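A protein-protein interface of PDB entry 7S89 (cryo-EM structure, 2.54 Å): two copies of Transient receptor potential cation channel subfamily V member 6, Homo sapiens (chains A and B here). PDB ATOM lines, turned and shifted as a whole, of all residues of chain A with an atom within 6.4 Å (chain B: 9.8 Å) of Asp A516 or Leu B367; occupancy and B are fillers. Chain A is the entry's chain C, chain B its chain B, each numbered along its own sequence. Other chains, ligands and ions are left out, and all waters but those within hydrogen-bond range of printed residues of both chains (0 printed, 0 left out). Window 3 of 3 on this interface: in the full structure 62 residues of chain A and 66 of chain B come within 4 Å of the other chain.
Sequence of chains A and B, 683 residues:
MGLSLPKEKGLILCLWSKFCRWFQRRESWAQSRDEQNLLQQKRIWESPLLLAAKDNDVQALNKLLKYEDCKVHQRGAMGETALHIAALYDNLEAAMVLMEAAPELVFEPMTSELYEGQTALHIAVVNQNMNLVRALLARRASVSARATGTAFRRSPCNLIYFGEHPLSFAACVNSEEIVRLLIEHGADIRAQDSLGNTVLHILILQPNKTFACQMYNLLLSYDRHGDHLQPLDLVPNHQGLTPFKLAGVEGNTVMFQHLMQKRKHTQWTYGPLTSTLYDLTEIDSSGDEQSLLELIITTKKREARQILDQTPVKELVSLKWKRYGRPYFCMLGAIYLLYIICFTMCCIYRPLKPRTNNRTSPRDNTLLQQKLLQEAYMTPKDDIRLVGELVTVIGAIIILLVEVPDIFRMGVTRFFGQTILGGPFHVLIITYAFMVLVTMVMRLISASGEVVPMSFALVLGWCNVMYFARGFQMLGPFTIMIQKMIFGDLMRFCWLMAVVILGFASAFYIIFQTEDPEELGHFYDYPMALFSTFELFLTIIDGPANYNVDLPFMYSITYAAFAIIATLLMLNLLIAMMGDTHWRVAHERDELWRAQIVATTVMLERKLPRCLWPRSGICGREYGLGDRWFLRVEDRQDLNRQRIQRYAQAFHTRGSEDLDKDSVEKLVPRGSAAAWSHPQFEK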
ATOM      1  N   PHE A 512      23.331  -4.018 -19.749  1.00  0.00           N
ATOM      2  CA  PHE A 512      23.252  -5.217 -20.566  1.00  0.00           C
ATOM      3  C   PHE A 512      21.909  -5.907 -20.477  1.00  0.00           C
ATOM      4  O   PHE A 512      21.782  -7.042 -20.928  1.00  0.00           O
ATOM      5  CB  PHE A 512      24.367  -6.177 -20.180  1.00  0.00           C
ATOM      6  CG  PHE A 512      25.705  -5.725 -20.630  1.00  0.00           C
ATOM      7  CD1 PHE A 512      26.132  -5.978 -21.912  1.00  0.00           C
ATOM      8  CD2 PHE A 512      26.519  -5.003 -19.791  1.00  0.00           C
ATOM      9  CE1 PHE A 512      27.364  -5.544 -22.339  1.00  0.00           C
ATOM     10  CE2 PHE A 512      27.740  -4.576 -20.205  1.00  0.00           C
ATOM     11  CZ  PHE A 512      28.164  -4.846 -21.477  1.00  0.00           C
ATOM     12  N   THR A 514      19.114  -5.186 -21.967  1.00  0.00           N
ATOM     13  CA  THR A 514      18.540  -5.232 -23.301  1.00  0.00           C
ATOM     14  C   THR A 514      19.392  -5.997 -24.305  1.00  0.00           C
ATOM     15  O   THR A 514      19.007  -6.092 -25.468  1.00  0.00           O
ATOM     16  CB  THR A 514      18.311  -3.804 -23.808  1.00  0.00           C
ATOM     17  OG1 THR A 514      19.534  -3.067 -23.739  1.00  0.00           O
ATOM     18  CG2 THR A 514      17.273  -3.106 -22.986  1.00  0.00           C
ATOM     19  N   GLU A 515      20.532  -6.535 -23.899  1.00  0.00           N
ATOM     20  CA  GLU A 515      21.468  -7.155 -24.824  1.00  0.00           C
ATOM     21  C   GLU A 515      21.294  -8.669 -24.817  1.00  0.00           C
ATOM     22  O   GLU A 515      20.566  -9.230 -24.002  1.00  0.00           O
ATOM     23  CB  GLU A 515      22.900  -6.767 -24.461  1.00  0.00           C
ATOM     24  CG  GLU A 515      23.087  -5.275 -24.399  1.00  0.00           C
ATOM     25  CD  GLU A 515      22.857  -4.592 -25.726  1.00  0.00           C
ATOM     26  OE1 GLU A 515      23.295  -5.123 -26.761  1.00  0.00           O
ATOM     27  OE2 GLU A 515      22.196  -3.541 -25.748  1.00  0.00           O
ATOM     28  N   ASP A 516      21.956  -9.326 -25.752  1.00  0.00           N
ATOM     29  CA  ASP A 516      21.923 -10.781 -25.821  1.00  0.00           C
ATOM     30  C   ASP A 516      22.991 -11.355 -24.898  1.00  0.00           C
ATOM     31  O   ASP A 516      24.163 -11.000 -25.036  1.00  0.00           O
ATOM     32  CB  ASP A 516      22.145 -11.239 -27.257  1.00  0.00           C
ATOM     33  CG  ASP A 516      21.878 -12.720 -27.474  1.00  0.00           C
ATOM     34  OD1 ASP A 516      21.404 -13.417 -26.568  1.00  0.00           O
ATOM     35  OD2 ASP A 516      22.167 -13.206 -28.579  1.00  0.00           O
ATOM     36  N   PRO A 517      22.635 -12.220 -23.943  1.00  0.00           N
ATOM     37  CA  PRO A 517      23.653 -12.745 -23.022  1.00  0.00           C
ATOM     38  C   PRO A 517      24.626 -13.707 -23.657  1.00  0.00           C
ATOM     39  O   PRO A 517      25.675 -13.972 -23.061  1.00  0.00           O
ATOM     40  CB  PRO A 517      22.816 -13.449 -21.952  1.00  0.00           C
ATOM     41  CG  PRO A 517      21.500 -12.862 -22.050  1.00  0.00           C
ATOM     42  CD  PRO A 517      21.281 -12.546 -23.475  1.00  0.00           C
ATOM     43  N   GLU A 518      24.300 -14.268 -24.826  1.00  0.00           N
ATOM     44  CA  GLU A 518      25.169 -15.260 -25.450  1.00  0.00           C
ATOM     45  C   GLU A 518      26.483 -14.641 -25.891  1.00  0.00           C
ATOM     46  O   GLU A 518      27.513 -15.319 -25.944  1.00  0.00           O
ATOM     47  CB  GLU A 518      24.465 -15.906 -26.635  1.00  0.00           C
ATOM     48  CG  GLU A 518      23.249 -16.710 -26.247  1.00  0.00           C
ATOM     49  CD  GLU A 518      23.592 -17.933 -25.421  1.00  0.00           C
ATOM     50  OE1 GLU A 518      24.651 -18.551 -25.662  1.00  0.00           O
ATOM     51  OE2 GLU A 518      22.806 -18.272 -24.513  1.00  0.00           O
ATOM     52  N   GLU A 519      26.464 -13.354 -26.207  1.00  0.00           N
ATOM     53  CA  GLU A 519      27.695 -12.659 -26.536  1.00  0.00           C
ATOM     54  C   GLU A 519      28.440 -12.215 -25.289  1.00  0.00           C
ATOM     55  O   GLU A 519      29.640 -12.471 -25.154  1.00  0.00           O
ATOM     56  CB  GLU A 519      27.392 -11.484 -27.455  1.00  0.00           C
ATOM     57  CG  GLU A 519      27.252 -11.903 -28.893  1.00  0.00           C
ATOM     58  CD  GLU A 519      25.894 -12.375 -29.252  1.00  0.00           C
ATOM     59  OE1 GLU A 519      24.999 -12.280 -28.400  1.00  0.00           O
ATOM     60  OE2 GLU A 519      25.717 -12.849 -30.393  1.00  0.00           O
ATOM     61  N   LEU A 520      27.756 -11.561 -24.360  1.00  0.00           N
ATOM     62  CA  LEU A 520      28.412 -11.094 -23.144  1.00  0.00           C
ATOM     63  C   LEU A 520      27.490 -11.369 -21.968  1.00  0.00           C
ATOM     64  O   LEU A 520      26.573 -10.592 -21.704  1.00  0.00           O
ATOM     65  CB  LEU A 520      28.773  -9.617 -23.270  1.00  0.00           C
ATOM     66  CG  LEU A 520      29.772  -9.020 -22.293  1.00  0.00           C
ATOM     67  CD1 LEU A 520      30.599  -7.992 -23.010  1.00  0.00           C
ATOM     68  CD2 LEU A 520      29.116  -8.468 -21.020  1.00  0.00           C
ATOM     69  N   GLY A 521      27.756 -12.458 -21.251  1.00  0.00           N
ATOM     70  CA  GLY A 521      26.882 -12.935 -20.205  1.00  0.00           C
ATOM     71  C   GLY A 521      27.365 -12.719 -18.796  1.00  0.00           C
ATOM     72  O   GLY A 521      26.895 -13.415 -17.890  1.00  0.00           O
ATOM     73  N   LEU B 352      10.651  -3.292 -19.975  1.00  0.00           N
ATOM     74  CA  LEU B 352      11.352  -3.717 -21.177  1.00  0.00           C
ATOM     75  C   LEU B 352      10.503  -4.716 -21.944  1.00  0.00           C
ATOM     76  O   LEU B 352       9.813  -5.540 -21.345  1.00  0.00           O
ATOM     77  CB  LEU B 352      12.718  -4.314 -20.809  1.00  0.00           C
ATOM     78  CG  LEU B 352      13.997  -3.482 -20.910  1.00  0.00           C
ATOM     79  CD1 LEU B 352      13.921  -2.177 -20.232  1.00  0.00           C
ATOM     80  CD2 LEU B 352      15.063  -4.261 -20.214  1.00  0.00           C
ATOM     81  N   LYS B 353      10.532  -4.620 -23.264  1.00  0.00           N
ATOM     82  CA  LYS B 353       9.772  -5.477 -24.160  1.00  0.00           C
ATOM     83  C   LYS B 353      10.686  -5.963 -25.271  1.00  0.00           C
ATOM     84  O   LYS B 353      11.742  -5.369 -25.506  1.00  0.00           O
ATOM     85  CB  LYS B 353       8.573  -4.719 -24.753  1.00  0.00           C
ATOM     86  CG  LYS B 353       8.952  -3.593 -25.672  1.00  0.00           C
ATOM     87  CD  LYS B 353       7.741  -2.855 -26.144  1.00  0.00           C
ATOM     88  CE  LYS B 353       8.124  -1.759 -27.089  1.00  0.00           C
ATOM     89  NZ  LYS B 353       6.941  -1.024 -27.572  1.00  0.00           N
ATOM     90  N   PRO B 354      10.332  -7.064 -25.947  1.00  0.00           N
ATOM     91  CA  PRO B 354      11.097  -7.483 -27.130  1.00  0.00           C
ATOM     92  C   PRO B 354      11.110  -6.432 -28.226  1.00  0.00           C
ATOM     93  O   PRO B 354      10.137  -5.706 -28.425  1.00  0.00           O
ATOM     94  CB  PRO B 354      10.370  -8.750 -27.582  1.00  0.00           C
ATOM     95  CG  PRO B 354       9.822  -9.294 -26.358  1.00  0.00           C
ATOM     96  CD  PRO B 354       9.409  -8.131 -25.518  1.00  0.00           C
ATOM     97  N   ARG B 355      12.239  -6.361 -28.928  1.00  0.00           N
ATOM     98  CA  ARG B 355      12.451  -5.327 -29.929  1.00  0.00           C
ATOM     99  C   ARG B 355      11.507  -5.504 -31.113  1.00  0.00           C
ATOM    100  O   ARG B 355      11.145  -6.623 -31.483  1.00  0.00           O
ATOM    101  CB  ARG B 355      13.906  -5.324 -30.399  1.00  0.00           C
ATOM    102  CG  ARG B 355      14.349  -6.549 -31.169  1.00  0.00           C
ATOM    103  CD  ARG B 355      15.767  -6.404 -31.638  1.00  0.00           C
ATOM    104  NE  ARG B 355      15.900  -5.268 -32.536  1.00  0.00           N
ATOM    105  CZ  ARG B 355      17.058  -4.724 -32.879  1.00  0.00           C
ATOM    106  NH1 ARG B 355      17.088  -3.684 -33.694  1.00  0.00           N
ATOM    107  NH2 ARG B 355      18.185  -5.221 -32.406  1.00  0.00           N
ATOM    108  N   THR B 356      11.066  -4.378 -31.666  1.00  0.00           N
ATOM    109  CA  THR B 356      10.103  -4.415 -32.756  1.00  0.00           C
ATOM    110  C   THR B 356      10.794  -4.537 -34.107  1.00  0.00           C
ATOM    111  O   THR B 356      10.437  -5.403 -34.914  1.00  0.00           O
ATOM    112  CB  THR B 356       9.220  -3.172 -32.703  1.00  0.00           C
ATOM    113  OG1 THR B 356      10.039  -2.001 -32.740  1.00  0.00           O
ATOM    114  CG2 THR B 356       8.403  -3.171 -31.436  1.00  0.00           C
ATOM    115  N   ASN B 357      11.797  -3.708 -34.365  1.00  0.00           N
ATOM    116  CA  ASN B 357      12.492  -3.764 -35.638  1.00  0.00           C
ATOM    117  C   ASN B 357      13.440  -4.960 -35.696  1.00  0.00           C
ATOM    118  O   ASN B 357      13.633  -5.692 -34.726  1.00  0.00           O
ATOM    119  CB  ASN B 357      13.242  -2.459 -35.912  1.00  0.00           C
ATOM    120  CG  ASN B 357      14.197  -2.071 -34.799  1.00  0.00           C
ATOM    121  OD1 ASN B 357      14.303  -2.744 -33.777  1.00  0.00           O
ATOM    122  ND2 ASN B 357      14.912  -0.976 -35.007  1.00  0.00           N
ATOM    123  N   ASN B 358      14.018  -5.163 -36.867  1.00  0.00           N
ATOM    124  CA  ASN B 358      14.898  -6.295 -37.062  1.00  0.00           C
ATOM    125  C   ASN B 358      16.343  -5.894 -36.805  1.00  0.00           C
ATOM    126  O   ASN B 358      16.685  -4.712 -36.707  1.00  0.00           O
ATOM    127  CB  ASN B 358      14.734  -6.857 -38.470  1.00  0.00           C
ATOM    128  CG  ASN B 358      13.331  -7.365 -38.726  1.00  0.00           C
ATOM    129  OD1 ASN B 358      12.591  -6.798 -39.528  1.00  0.00           O
ATOM    130  ND2 ASN B 358      12.955  -8.438 -38.040  1.00  0.00           N
ATOM    131  N   ARG B 359      17.189  -6.908 -36.678  1.00  0.00           N
ATOM    132  CA  ARG B 359      18.602  -6.686 -36.429  1.00  0.00           C
ATOM    133  C   ARG B 359      19.261  -6.083 -37.662  1.00  0.00           C
ATOM    134  O   ARG B 359      19.258  -6.686 -38.739  1.00  0.00           O
ATOM    135  CB  ARG B 359      19.260  -8.009 -36.051  1.00  0.00           C
ATOM    136  CG  ARG B 359      20.633  -7.854 -35.520  1.00  0.00           C
ATOM    137  CD  ARG B 359      21.258  -9.157 -35.088  1.00  0.00           C
ATOM    138  NE  ARG B 359      21.568 -10.031 -36.205  1.00  0.00           N
ATOM    139  CZ  ARG B 359      22.010 -11.271 -36.060  1.00  0.00           C
ATOM    140  NH1 ARG B 359      22.197 -11.762 -34.843  1.00  0.00           N
ATOM    141  NH2 ARG B 359      22.274 -12.016 -37.125  1.00  0.00           N
ATOM    142  N   PRO B 362      25.061  -7.596 -38.221  1.00  0.00           N
ATOM    143  CA  PRO B 362      25.448  -8.660 -37.278  1.00  0.00           C
ATOM    144  C   PRO B 362      26.110  -8.145 -36.009  1.00  0.00           C
ATOM    145  O   PRO B 362      26.143  -8.869 -35.006  1.00  0.00           O
ATOM    146  CB  PRO B 362      26.407  -9.524 -38.105  1.00  0.00           C
ATOM    147  CG  PRO B 362      26.008  -9.285 -39.493  1.00  0.00           C
ATOM    148  CD  PRO B 362      25.592  -7.858 -39.566  1.00  0.00           C
ATOM    149  N   ARG B 363      26.643  -6.919 -36.018  1.00  0.00           N
ATOM    150  CA  ARG B 363      27.201  -6.344 -34.799  1.00  0.00           C
ATOM    151  C   ARG B 363      26.119  -5.869 -33.842  1.00  0.00           C
ATOM    152  O   ARG B 363      26.410  -5.592 -32.676  1.00  0.00           O
ATOM    153  CB  ARG B 363      28.143  -5.193 -35.134  1.00  0.00           C
ATOM    154  CG  ARG B 363      29.353  -5.622 -35.913  1.00  0.00           C
ATOM    155  CD  ARG B 363      30.300  -4.480 -36.102  1.00  0.00           C
ATOM    156  NE  ARG B 363      30.820  -4.050 -34.813  1.00  0.00           N
ATOM    157  CZ  ARG B 363      31.863  -4.595 -34.210  1.00  0.00           C
ATOM    158  NH1 ARG B 363      32.512  -5.596 -34.772  1.00  0.00           N
ATOM    159  NH2 ARG B 363      32.241  -4.143 -33.036  1.00  0.00           N
ATOM    160  N   ASP B 364      24.884  -5.740 -34.316  1.00  0.00           N
ATOM    161  CA  ASP B 364      23.778  -5.342 -33.461  1.00  0.00           C
ATOM    162  C   ASP B 364      23.446  -6.460 -32.482  1.00  0.00           C
ATOM    163  O   ASP B 364      23.092  -7.569 -32.881  1.00  0.00           O
ATOM    164  CB  ASP B 364      22.563  -5.006 -34.322  1.00  0.00           C
ATOM    165  CG  ASP B 364      21.453  -4.338 -33.550  1.00  0.00           C
ATOM    166  OD1 ASP B 364      21.614  -4.045 -32.352  1.00  0.00           O
ATOM    167  OD2 ASP B 364      20.388  -4.117 -34.148  1.00  0.00           O
ATOM    168  N   ASN B 365      23.535  -6.156 -31.193  1.00  0.00           N
ATOM    169  CA  ASN B 365      23.384  -7.165 -30.161  1.00  0.00           C
ATOM    170  C   ASN B 365      22.102  -7.001 -29.362  1.00  0.00           C
ATOM    171  O   ASN B 365      21.804  -7.846 -28.518  1.00  0.00           O
ATOM    172  CB  ASN B 365      24.567  -7.113 -29.190  1.00  0.00           C
ATOM    173  CG  ASN B 365      24.841  -8.439 -28.548  1.00  0.00           C
ATOM    174  OD1 ASN B 365      25.614  -8.528 -27.608  1.00  0.00           O
ATOM    175  ND2 ASN B 365      24.306  -9.491 -29.128  1.00  0.00           N
ATOM    176  N   THR B 366      21.347  -5.941 -29.604  1.00  0.00           N
ATOM    177  CA  THR B 366      20.213  -5.591 -28.765  1.00  0.00           C
ATOM    178  C   THR B 366      19.038  -6.528 -29.014  1.00  0.00           C
ATOM    179  O   THR B 366      18.679  -6.797 -30.161  1.00  0.00           O
ATOM    180  CB  THR B 366      19.825  -4.144 -29.048  1.00  0.00           C
ATOM    181  OG1 THR B 366      20.970  -3.309 -28.869  1.00  0.00           O
ATOM    182  CG2 THR B 366      18.759  -3.683 -28.119  1.00  0.00           C
ATOM    183  N   LEU B 367      18.454  -7.050 -27.937  1.00  0.00           N
ATOM    184  CA  LEU B 367      17.300  -7.929 -28.022  1.00  0.00           C
ATOM    185  C   LEU B 367      16.029  -7.298 -27.499  1.00  0.00           C
ATOM    186  O   LEU B 367      14.940  -7.754 -27.853  1.00  0.00           O
ATOM    187  CB  LEU B 367      17.526  -9.217 -27.221  1.00  0.00           C
ATOM    188  CG  LEU B 367      18.415 -10.324 -27.765  1.00  0.00           C
ATOM    189  CD1 LEU B 367      18.390 -11.445 -26.771  1.00  0.00           C
ATOM    190  CD2 LEU B 367      17.947 -10.808 -29.112  1.00  0.00           C
ATOM    191  N   LEU B 368      16.135  -6.288 -26.653  1.00  0.00           N
ATOM    192  CA  LEU B 368      15.007  -5.752 -25.926  1.00  0.00           C
ATOM    193  C   LEU B 368      15.024  -4.251 -26.088  1.00  0.00           C
ATOM    194  O   LEU B 368      16.064  -3.650 -26.332  1.00  0.00           O
ATOM    195  CB  LEU B 368      15.079  -6.091 -24.439  1.00  0.00           C
ATOM    196  CG  LEU B 368      14.913  -7.537 -24.004  1.00  0.00           C
ATOM    197  CD1 LEU B 368      15.007  -7.594 -22.505  1.00  0.00           C
ATOM    198  CD2 LEU B 368      13.606  -8.099 -24.448  1.00  0.00           C
ATOM    199  N   GLN B 369      13.870  -3.636 -25.946  1.00  0.00           N
ATOM    200  CA  GLN B 369      13.827  -2.192 -25.878  1.00  0.00           C
ATOM    201  C   GLN B 369      12.878  -1.788 -24.774  1.00  0.00           C
ATOM    202  O   GLN B 369      12.107  -2.599 -24.263  1.00  0.00           O
ATOM    203  CB  GLN B 369      13.417  -1.564 -27.202  1.00  0.00           C
ATOM    204  CG  GLN B 369      12.022  -1.857 -27.624  1.00  0.00           C
ATOM    205  CD  GLN B 369      11.719  -1.243 -28.960  1.00  0.00           C
ATOM    206  OE1 GLN B 369      12.566  -0.589 -29.558  1.00  0.00           O
ATOM    207  NE2 GLN B 369      10.508  -1.439 -29.437  1.00  0.00           N
ATOM    208  N   GLN B 370      12.963  -0.528 -24.386  1.00  0.00           N
ATOM    209  CA  GLN B 370      12.127  -0.065 -23.296  1.00  0.00           C
ATOM    210  C   GLN B 370      10.712   0.183 -23.798  1.00  0.00           C
ATOM    211  O   GLN B 370      10.499   0.536 -24.959  1.00  0.00           O
ATOM    212  CB  GLN B 370      12.736   1.176 -22.656  1.00  0.00           C
ATOM    213  CG  GLN B 370      12.697   2.427 -23.458  1.00  0.00           C
ATOM    214  CD  GLN B 370      13.538   3.498 -22.825  1.00  0.00           C
ATOM    215  OE1 GLN B 370      14.303   3.234 -21.907  1.00  0.00           O
ATOM    216  NE2 GLN B 370      13.341   4.725 -23.252  1.00  0.00           N
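The guanidinium group (NH2) of Arg B355 sits at hydrogen-bond distance from the backbone carbonyl oxygen (O) of Thr B366 (2.8 Å).
The backbone NH (N) of Arg B355 lies within hydrogen-bond range of the backbone carbonyl oxygen (O) of Leu B367 (3.2 Å).
OD1 of Asp B364 lies within hydrogen-bond range of N of Thr B366.
OG1 of Thr A514 lies within hydrogen-bond range of OE2 of Glu A515, 3.4 Å away.
N of Glu A518 sits close to OD1 of Asp A516 (3.5 Å).
Printed residues of chain B within 4 Å of Thr A514: Leu B352, Thr B366, Leu B367 and Leu B368.
Glu A515 touches just these residues of chain B: Asn B365 and Thr B366.
Of the printed residues of chain B, Asp A516 touches Asn B365 (3.1 Å) and Leu B367 (3.6 Å).
Of chain B, only Asn B365 (3.0 Å) comes within 4 Å of Glu A519.
Printed residues of chain A within 4 Å of Leu B352: Thr A514.
Arg B355 touches none of the printed residues of chain A.
Printed residues of chain A within 4 Å of Thr B366: Thr A514 (3.5 Å) and Glu A515 (3.4 Å).
Leu B367 touches two residues of chain A.
Printed residues of chain A within 4 Å of Leu B368: Thr A514 (3.1 Å).
Of the 17 printed residues of chain B, 5 touch a printed residue of chain A.
Hydrophobic or aromatic side chains of chain B that line the printed part of chain A: Leu B352, Leu B367 and Leu B368.
Among the printed residues, no Asp or Glu carboxylate lies within 4 Å of a Lys or Arg side-chain nitrogen of the other chain.
No position is printed for both chains.
The backbone carbonyl oxygen (O) of Asn B365 is in hydrogen-bond range of the backbone NH (N) of Asp A516, 3.1 Å away.
The side-chain amide nitrogen of Asn B365 is in hydrogen-bond range of the side-chain carboxylate of Glu A519 (3.0 Å).
The side-chain hydroxyl (OG1) of Thr B366 lies within hydrogen-bond range of the side-chain carboxylate (OE2) of Glu A515 (3.4 Å).
The backbone carbonyl oxygen (O) of Thr A514 is in hydrogen-bond range of the backbone NH (N) of Leu B367.
The backbone NH of Leu B368 is in hydrogen-bond range of the backbone carbonyl oxygen of Thr A514.
Among the printed residues, pairs that only touch across the chains: Thr A514 with Leu B352, Thr A514 with Thr B366, Glu A515 with Asn B365 and Asp A516 with Leu B367.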
